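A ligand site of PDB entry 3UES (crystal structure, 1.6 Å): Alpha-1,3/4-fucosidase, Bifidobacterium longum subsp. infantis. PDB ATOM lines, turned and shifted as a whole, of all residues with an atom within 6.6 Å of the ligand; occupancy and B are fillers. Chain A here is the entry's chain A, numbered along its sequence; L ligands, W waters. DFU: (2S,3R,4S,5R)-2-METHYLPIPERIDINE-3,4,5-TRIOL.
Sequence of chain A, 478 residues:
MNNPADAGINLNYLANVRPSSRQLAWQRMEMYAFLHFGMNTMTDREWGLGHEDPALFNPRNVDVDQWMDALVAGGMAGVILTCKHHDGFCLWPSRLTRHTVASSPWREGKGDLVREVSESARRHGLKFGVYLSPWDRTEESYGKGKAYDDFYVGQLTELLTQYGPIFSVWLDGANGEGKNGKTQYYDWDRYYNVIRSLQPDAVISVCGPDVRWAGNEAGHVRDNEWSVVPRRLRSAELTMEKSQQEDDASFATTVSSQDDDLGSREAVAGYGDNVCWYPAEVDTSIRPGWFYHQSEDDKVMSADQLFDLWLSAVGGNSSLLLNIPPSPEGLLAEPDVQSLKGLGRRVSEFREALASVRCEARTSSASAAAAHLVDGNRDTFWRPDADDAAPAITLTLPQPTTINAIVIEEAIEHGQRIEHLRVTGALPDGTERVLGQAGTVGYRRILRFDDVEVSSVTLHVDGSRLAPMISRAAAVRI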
ATOM      1  N   PHE A  34       7.745   6.090 -13.369  1.00  0.00           N
ATOM      2  CA  PHE A  34       9.057   5.427 -13.596  1.00  0.00           C
ATOM      3  C   PHE A  34       9.236   4.450 -12.455  1.00  0.00           C
ATOM      4  O   PHE A  34       8.802   4.745 -11.316  1.00  0.00           O
ATOM      5  CB  PHE A  34      10.094   6.525 -13.447  1.00  0.00           C
ATOM      6  CG  PHE A  34      11.075   6.725 -14.633  1.00  0.00           C
ATOM      7  CD1 PHE A  34      11.392   5.686 -15.524  1.00  0.00           C
ATOM      8  CD2 PHE A  34      11.638   7.989 -14.826  1.00  0.00           C
ATOM      9  CE1 PHE A  34      12.378   5.902 -16.540  1.00  0.00           C
ATOM     10  CE2 PHE A  34      12.641   8.208 -15.795  1.00  0.00           C
ATOM     11  CZ  PHE A  34      12.954   7.167 -16.699  1.00  0.00           C
ATOM     12  N   HIS A  36      12.570   2.760 -11.145  1.00  0.00           N
ATOM     13  CA  HIS A  36      13.991   2.420 -11.155  1.00  0.00           C
ATOM     14  C   HIS A  36      14.205   1.240 -10.176  1.00  0.00           C
ATOM     15  O   HIS A  36      14.012   1.403  -8.903  1.00  0.00           O
ATOM     16  CB  HIS A  36      14.872   3.595 -10.729  1.00  0.00           C
ATOM     17  CG  HIS A  36      15.135   4.572 -11.839  1.00  0.00           C
ATOM     18  ND1 HIS A  36      14.095   5.312 -12.372  1.00  0.00           N
ATOM     19  CD2 HIS A  36      16.239   4.908 -12.556  1.00  0.00           C
ATOM     20  CE1 HIS A  36      14.568   6.103 -13.408  1.00  0.00           C
ATOM     21  NE2 HIS A  36      15.850   5.873 -13.505  1.00  0.00           N
ATOM     22  N   ASN A  40      21.188  -1.804  -8.657  1.00  0.00           N
ATOM     23  CA  ASN A  40      21.444  -0.716  -7.735  1.00  0.00           C
ATOM     24  C   ASN A  40      20.546  -0.742  -6.502  1.00  0.00           C
ATOM     25  O   ASN A  40      20.938  -0.180  -5.472  1.00  0.00           O
ATOM     26  CB  ASN A  40      21.215   0.633  -8.466  1.00  0.00           C
ATOM     27  CG  ASN A  40      22.262   0.917  -9.564  1.00  0.00           C
ATOM     28  OD1 ASN A  40      23.216   0.133  -9.860  1.00  0.00           O
ATOM     29  ND2 ASN A  40      22.072   2.073 -10.210  1.00  0.00           N
ATOM     30  N   GLU A  46      23.173   4.847  -6.656  1.00  0.00           N
ATOM     31  CA  GLU A  46      22.438   5.553  -7.737  1.00  0.00           C
ATOM     32  C   GLU A  46      22.937   5.166  -9.057  1.00  0.00           C
ATOM     33  O   GLU A  46      22.109   5.058 -10.020  1.00  0.00           O
ATOM     34  CB  GLU A  46      22.574   7.088  -7.564  1.00  0.00           C
ATOM     35  CG  GLU A  46      21.509   7.529  -6.475  1.00  0.00           C
ATOM     36  CD  GLU A  46      20.080   7.401  -6.949  1.00  0.00           C
ATOM     37  OE1 GLU A  46      19.737   8.129  -7.942  1.00  0.00           O
ATOM     38  OE2 GLU A  46      19.369   6.498  -6.434  1.00  0.00           O
ATOM     39  N   TRP A  47      24.274   5.123  -9.283  1.00  0.00           N
ATOM     40  CA  TRP A  47      24.781   4.528 -10.551  1.00  0.00           C
ATOM     41  C   TRP A  47      25.686   3.384 -10.101  1.00  0.00           C
ATOM     42  O   TRP A  47      26.561   3.554  -9.176  1.00  0.00           O
ATOM     43  CB  TRP A  47      25.689   5.503 -11.222  1.00  0.00           C
ATOM     44  CG  TRP A  47      25.047   6.598 -11.937  1.00  0.00           C
ATOM     45  CD1 TRP A  47      23.656   6.853 -12.137  1.00  0.00           C
ATOM     46  CD2 TRP A  47      25.730   7.572 -12.763  1.00  0.00           C
ATOM     47  NE1 TRP A  47      23.497   7.950 -13.031  1.00  0.00           N
ATOM     48  CE2 TRP A  47      24.716   8.405 -13.394  1.00  0.00           C
ATOM     49  CE3 TRP A  47      27.055   7.844 -13.004  1.00  0.00           C
ATOM     50  CZ2 TRP A  47      25.087   9.475 -14.218  1.00  0.00           C
ATOM     51  CZ3 TRP A  47      27.453   8.864 -13.825  1.00  0.00           C
ATOM     52  CH2 TRP A  47      26.421   9.700 -14.497  1.00  0.00           C
ATOM     53  N   THR A  82      12.911   0.454 -15.678  1.00  0.00           N
ATOM     54  CA  THR A  82      14.353   0.375 -16.029  1.00  0.00           C
ATOM     55  C   THR A  82      14.667  -1.146 -16.313  1.00  0.00           C
ATOM     56  O   THR A  82      15.092  -1.893 -15.434  1.00  0.00           O
ATOM     57  CB  THR A  82      15.285   0.942 -14.940  1.00  0.00           C
ATOM     58  OG1 THR A  82      15.019   0.220 -13.690  1.00  0.00           O
ATOM     59  CG2 THR A  82      15.027   2.442 -14.783  1.00  0.00           C
ATOM     60  N   HIS A  85      19.698  -0.484 -16.522  1.00  0.00           N
ATOM     61  CA  HIS A  85      20.222   0.845 -16.229  1.00  0.00           C
ATOM     62  C   HIS A  85      21.713   0.937 -16.650  1.00  0.00           C
ATOM     63  O   HIS A  85      22.183   0.086 -17.444  1.00  0.00           O
ATOM     64  CB  HIS A  85      20.018   1.147 -14.718  1.00  0.00           C
ATOM     65  CG  HIS A  85      20.020   2.620 -14.419  1.00  0.00           C
ATOM     66  ND1 HIS A  85      21.135   3.286 -13.877  1.00  0.00           N
ATOM     67  CD2 HIS A  85      19.027   3.607 -14.660  1.00  0.00           C
ATOM     68  CE1 HIS A  85      20.861   4.594 -13.777  1.00  0.00           C
ATOM     69  NE2 HIS A  85      19.583   4.823 -14.275  1.00  0.00           N
ATOM     70  N   HIS A  86      22.387   2.017 -16.281  1.00  0.00           N
ATOM     71  CA  HIS A  86      23.709   2.251 -16.870  1.00  0.00           C
ATOM     72  C   HIS A  86      24.695   1.099 -16.445  1.00  0.00           C
ATOM     73  O   HIS A  86      25.664   0.834 -17.208  1.00  0.00           O
ATOM     74  CB  HIS A  86      24.307   3.493 -16.331  1.00  0.00           C
ATOM     75  CG  HIS A  86      23.496   4.749 -16.487  1.00  0.00           C
ATOM     76  ND1 HIS A  86      22.654   5.022 -17.540  1.00  0.00           N
ATOM     77  CD2 HIS A  86      23.399   5.855 -15.607  1.00  0.00           C
ATOM     78  CE1 HIS A  86      22.114   6.262 -17.376  1.00  0.00           C
ATOM     79  NE2 HIS A  86      22.588   6.797 -16.238  1.00  0.00           N
ATOM     80  N   TYR A 131      12.712   1.446 -20.416  1.00  0.00           N
ATOM     81  CA  TYR A 131      13.932   2.187 -20.351  1.00  0.00           C
ATOM     82  C   TYR A 131      15.083   1.224 -20.601  1.00  0.00           C
ATOM     83  O   TYR A 131      15.197   0.198 -19.861  1.00  0.00           O
ATOM     84  CB  TYR A 131      14.007   2.776 -18.921  1.00  0.00           C
ATOM     85  CG  TYR A 131      15.297   3.493 -18.576  1.00  0.00           C
ATOM     86  CD1 TYR A 131      15.336   4.857 -18.401  1.00  0.00           C
ATOM     87  CD2 TYR A 131      16.479   2.794 -18.364  1.00  0.00           C
ATOM     88  CE1 TYR A 131      16.473   5.539 -18.021  1.00  0.00           C
ATOM     89  CE2 TYR A 131      17.651   3.447 -17.997  1.00  0.00           C
ATOM     90  CZ  TYR A 131      17.650   4.807 -17.815  1.00  0.00           C
ATOM     91  OH  TYR A 131      18.827   5.439 -17.506  1.00  0.00           O
ATOM     92  N   TRP A 135      24.103   4.050 -22.352  1.00  0.00           N
ATOM     93  CA  TRP A 135      25.414   3.818 -21.658  1.00  0.00           C
ATOM     94  C   TRP A 135      25.367   2.480 -20.977  1.00  0.00           C
ATOM     95  O   TRP A 135      24.403   2.183 -20.245  1.00  0.00           O
ATOM     96  CB  TRP A 135      25.545   4.989 -20.715  1.00  0.00           C
ATOM     97  CG  TRP A 135      26.863   4.951 -19.984  1.00  0.00           C
ATOM     98  CD1 TRP A 135      28.068   4.531 -20.438  1.00  0.00           C
ATOM     99  CD2 TRP A 135      27.083   5.467 -18.660  1.00  0.00           C
ATOM    100  NE1 TRP A 135      29.029   4.635 -19.419  1.00  0.00           N
ATOM    101  CE2 TRP A 135      28.540   5.246 -18.351  1.00  0.00           C
ATOM    102  CE3 TRP A 135      26.269   6.088 -17.710  1.00  0.00           C
ATOM    103  CZ2 TRP A 135      29.072   5.642 -17.100  1.00  0.00           C
ATOM    104  CZ3 TRP A 135      26.804   6.403 -16.449  1.00  0.00           C
ATOM    105  CH2 TRP A 135      28.196   6.239 -16.185  1.00  0.00           C
ATOM    106  N   TRP A 170      12.409   4.755 -23.721  1.00  0.00           N
ATOM    107  CA  TRP A 170      12.997   5.900 -23.042  1.00  0.00           C
ATOM    108  C   TRP A 170      14.509   5.724 -23.165  1.00  0.00           C
ATOM    109  O   TRP A 170      15.066   4.728 -22.629  1.00  0.00           O
ATOM    110  CB  TRP A 170      12.547   5.854 -21.607  1.00  0.00           C
ATOM    111  CG  TRP A 170      12.457   7.277 -21.008  1.00  0.00           C
ATOM    112  CD1 TRP A 170      11.299   8.047 -21.023  1.00  0.00           C
ATOM    113  CD2 TRP A 170      13.464   8.082 -20.279  1.00  0.00           C
ATOM    114  NE1 TRP A 170      11.536   9.273 -20.370  1.00  0.00           N
ATOM    115  CE2 TRP A 170      12.824   9.309 -19.868  1.00  0.00           C
ATOM    116  CE3 TRP A 170      14.806   7.898 -19.987  1.00  0.00           C
ATOM    117  CZ2 TRP A 170      13.480  10.293 -19.097  1.00  0.00           C
ATOM    118  CZ3 TRP A 170      15.497   8.896 -19.201  1.00  0.00           C
ATOM    119  CH2 TRP A 170      14.851  10.052 -18.794  1.00  0.00           C
ATOM    120  N   ASP A 172      17.935   7.227 -22.438  1.00  0.00           N
ATOM    121  CA  ASP A 172      18.624   8.211 -21.579  1.00  0.00           C
ATOM    122  C   ASP A 172      19.911   8.682 -22.212  1.00  0.00           C
ATOM    123  O   ASP A 172      20.694   7.841 -22.706  1.00  0.00           O
ATOM    124  CB  ASP A 172      18.969   7.505 -20.250  1.00  0.00           C
ATOM    125  CG  ASP A 172      19.128   8.506 -19.064  1.00  0.00           C
ATOM    126  OD1 ASP A 172      19.605   9.630 -19.264  1.00  0.00           O
ATOM    127  OD2 ASP A 172      18.762   8.086 -17.897  1.00  0.00           O
ATOM    128  N   GLY A 173      20.127  10.013 -22.201  1.00  0.00           N
ATOM    129  CA  GLY A 173      21.400  10.502 -22.772  1.00  0.00           C
ATOM    130  C   GLY A 173      22.521  10.573 -21.706  1.00  0.00           C
ATOM    131  O   GLY A 173      23.671  10.847 -22.142  1.00  0.00           O
ATOM    132  N   ALA A 174      22.275  10.247 -20.447  1.00  0.00           N
ATOM    133  CA  ALA A 174      23.302  10.357 -19.368  1.00  0.00           C
ATOM    134  C   ALA A 174      24.456   9.450 -19.715  1.00  0.00           C
ATOM    135  O   ALA A 174      24.353   8.287 -20.091  1.00  0.00           O
ATOM    136  CB  ALA A 174      22.762  10.014 -17.995  1.00  0.00           C
ATOM    137  N   ASN A 175      25.693  10.028 -19.573  1.00  0.00           N
ATOM    138  CA  ASN A 175      26.877   9.183 -19.800  1.00  0.00           C
ATOM    139  C   ASN A 175      28.054   9.671 -18.932  1.00  0.00           C
ATOM    140  O   ASN A 175      28.439  10.844 -18.992  1.00  0.00           O
ATOM    141  CB  ASN A 175      27.304   9.392 -21.242  1.00  0.00           C
ATOM    142  CG  ASN A 175      28.377   8.431 -21.635  1.00  0.00           C
ATOM    143  OD1 ASN A 175      29.466   8.549 -21.163  1.00  0.00           O
ATOM    144  ND2 ASN A 175      28.006   7.346 -22.368  1.00  0.00           N
ATOM    145  N   TRP A 213      13.206  15.609 -23.415  1.00  0.00           N
ATOM    146  CA  TRP A 213      13.551  15.767 -21.980  1.00  0.00           C
ATOM    147  C   TRP A 213      13.451  17.286 -21.659  1.00  0.00           C
ATOM    148  O   TRP A 213      14.061  18.067 -22.348  1.00  0.00           O
ATOM    149  CB  TRP A 213      14.971  15.291 -21.829  1.00  0.00           C
ATOM    150  CG  TRP A 213      15.461  15.516 -20.403  1.00  0.00           C
ATOM    151  CD1 TRP A 213      14.848  15.109 -19.236  1.00  0.00           C
ATOM    152  CD2 TRP A 213      16.674  16.220 -20.038  1.00  0.00           C
ATOM    153  NE1 TRP A 213      15.661  15.480 -18.161  1.00  0.00           N
ATOM    154  CE2 TRP A 213      16.751  16.170 -18.583  1.00  0.00           C
ATOM    155  CE3 TRP A 213      17.711  16.815 -20.778  1.00  0.00           C
ATOM    156  CZ2 TRP A 213      17.847  16.732 -17.873  1.00  0.00           C
ATOM    157  CZ3 TRP A 213      18.795  17.393 -20.091  1.00  0.00           C
ATOM    158  CH2 TRP A 213      18.855  17.356 -18.671  1.00  0.00           C
ATOM    159  N   GLU A 217      15.993  17.514 -13.784  1.00  0.00           N
ATOM    160  CA  GLU A 217      15.428  16.354 -13.181  1.00  0.00           C
ATOM    161  C   GLU A 217      14.949  16.674 -11.798  1.00  0.00           C
ATOM    162  O   GLU A 217      14.690  15.806 -11.004  1.00  0.00           O
ATOM    163  CB  GLU A 217      16.420  15.142 -13.299  1.00  0.00           C
ATOM    164  CG  GLU A 217      16.396  14.606 -14.789  1.00  0.00           C
ATOM    165  CD  GLU A 217      17.137  13.247 -15.028  1.00  0.00           C
ATOM    166  OE1 GLU A 217      18.240  13.081 -14.427  1.00  0.00           O
ATOM    167  OE2 GLU A 217      16.665  12.431 -15.867  1.00  0.00           O
ATOM    168  N   ASP A 283      10.681  14.835 -15.858  1.00  0.00           N
ATOM    169  CA  ASP A 283      10.903  13.566 -15.120  1.00  0.00           C
ATOM    170  C   ASP A 283      11.574  13.880 -13.735  1.00  0.00           C
ATOM    171  O   ASP A 283      12.545  14.653 -13.695  1.00  0.00           O
ATOM    172  CB  ASP A 283      11.793  12.581 -15.949  1.00  0.00           C
ATOM    173  CG  ASP A 283      13.209  13.038 -16.141  1.00  0.00           C
ATOM    174  OD1 ASP A 283      14.100  12.109 -15.897  1.00  0.00           O
ATOM    175  OD2 ASP A 283      13.501  14.165 -16.503  1.00  0.00           O
ATOM    176  N   TRP A 290      16.912   8.217  -7.510  1.00  0.00           N
ATOM    177  CA  TRP A 290      16.060   7.392  -8.367  1.00  0.00           C
ATOM    178  C   TRP A 290      15.882   6.002  -7.890  1.00  0.00           C
ATOM    179  O   TRP A 290      14.796   5.454  -7.990  1.00  0.00           O
ATOM    180  CB  TRP A 290      16.696   7.333  -9.793  1.00  0.00           C
ATOM    181  CG  TRP A 290      16.768   8.697 -10.390  1.00  0.00           C
ATOM    182  CD1 TRP A 290      17.850   9.533 -10.476  1.00  0.00           C
ATOM    183  CD2 TRP A 290      15.681   9.400 -11.097  1.00  0.00           C
ATOM    184  NE1 TRP A 290      17.539  10.672 -11.133  1.00  0.00           N
ATOM    185  CE2 TRP A 290      16.236  10.630 -11.538  1.00  0.00           C
ATOM    186  CE3 TRP A 290      14.339   9.068 -11.400  1.00  0.00           C
ATOM    187  CZ2 TRP A 290      15.507  11.561 -12.277  1.00  0.00           C
ATOM    188  CZ3 TRP A 290      13.583  10.032 -12.100  1.00  0.00           C
ATOM    189  CH2 TRP A 290      14.187  11.280 -12.515  1.00  0.00           C
ATOM    190  N   PHE A 291      16.942   5.402  -7.297  1.00  0.00           N
ATOM    191  CA  PHE A 291      16.750   4.035  -6.782  1.00  0.00           C
ATOM    192  C   PHE A 291      16.403   4.120  -5.274  1.00  0.00           C
ATOM    193  O   PHE A 291      16.474   5.170  -4.717  1.00  0.00           O
ATOM    194  CB  PHE A 291      18.063   3.200  -6.955  1.00  0.00           C
ATOM    195  CG  PHE A 291      18.268   2.795  -8.389  1.00  0.00           C
ATOM    196  CD1 PHE A 291      17.784   1.561  -8.800  1.00  0.00           C
ATOM    197  CD2 PHE A 291      18.932   3.649  -9.289  1.00  0.00           C
ATOM    198  CE1 PHE A 291      17.862   1.151 -10.139  1.00  0.00           C
ATOM    199  CE2 PHE A 291      19.004   3.305 -10.686  1.00  0.00           C
ATOM    200  CZ  PHE A 291      18.532   2.025 -11.068  1.00  0.00           C
HETATM  201  C1  DFU L   1      19.677  10.143 -15.745  1.00  0.00           C
HETATM  202  C2  DFU L   1      20.267   8.889 -15.100  1.00  0.00           C
HETATM  203  C3  DFU L   1      19.667   8.645 -13.730  1.00  0.00           C
HETATM  204  C4  DFU L   1      18.197   8.295 -13.919  1.00  0.00           C
HETATM  205  C5  DFU L   1      17.478   9.531 -14.625  1.00  0.00           C
HETATM  206  C6  DFU L   1      15.980   9.214 -14.949  1.00  0.00           C
HETATM  207  O4  DFU L   1      18.026   7.128 -14.675  1.00  0.00           O
HETATM  208  O3  DFU L   1      20.254   7.491 -13.053  1.00  0.00           O
HETATM  209  O2  DFU L   1      21.678   9.102 -14.959  1.00  0.00           O
HETATM  210  N5  DFU L   1      18.172   9.911 -15.858  1.00  0.00           N
HETATM  211  O   HOH W   1      22.495  11.782 -15.157  1.00  0.00           O
HETATM  212  O   HOH W   2      20.005   6.812 -10.411  1.00  0.00           O
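The side-chain carboxylate (OD2) of Asp 283 lies within hydrogen-bond range of the indole nitrogen (NE1) of Trp 213 (3.0 Å). The backbone NH (N) of Trp 290 sits at hydrogen-bond distance from the side-chain carboxylate (OE1) of Glu 46 (2.9 Å). The side-chain carboxylate (OD2) of Asp 172 sits at hydrogen-bond distance from the side-chain hydroxyl (OH) of Tyr 131, at 2.7 Å. The side-chain carboxylate (OE2) of Glu 217 sits close to the side-chain carboxylate (OD1) of Asp 283 (2.6 Å). A ring nitrogen (NE2) of His 85 lies within hydrogen-bond range of the side-chain hydroxyl (OH) of Tyr 131. The backbone NH of Ala 174 lies within hydrogen-bond range of the side-chain carboxylate of Asp 172.
Phe 34 touches the ligand (CE2 to C6, 3.6 Å). Ala 174 touches the ligand. Asp 283 touches the ligand (OD1 to C6, 3.6 Å). CE2 of Trp 290 touches C5 of the ligand, at 3.5 Å. Hydrophobic or aromatic side chains that line the ligand: Phe 34, His 36, Trp 47, His 85, His 86, Tyr 131, Ala 174 and Trp 290. Of the 20 residues printed, 11 come within 4 Å of the ligand.
Water W2 bridges O3 of the ligand (2.7 Å) and O of Glu 46 (2.8 Å).
O4 of the ligand is in hydrogen-bond range of NE2 of His 36. The side-chain hydroxyl of Tyr 131 lies within hydrogen-bond range of an oxygen (O4) of the ligand (3.4 Å). NE2 of His 86 is in hydrogen-bond range of O2 of the ligand. The side-chain carboxylate (OE2) of Glu 217 lies within salt-bridge range of a nitrogen (N5) of the ligand (2.9 Å). N5 of the ligand is in salt-bridge range of OD2 of Asp 172. O2 of the ligand is in hydrogen-bond range of NE1 of Trp 47. A ring nitrogen (NE2) of His 85 is in hydrogen-bond range of an oxygen (O4) of the ligand, 2.8 Å away.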
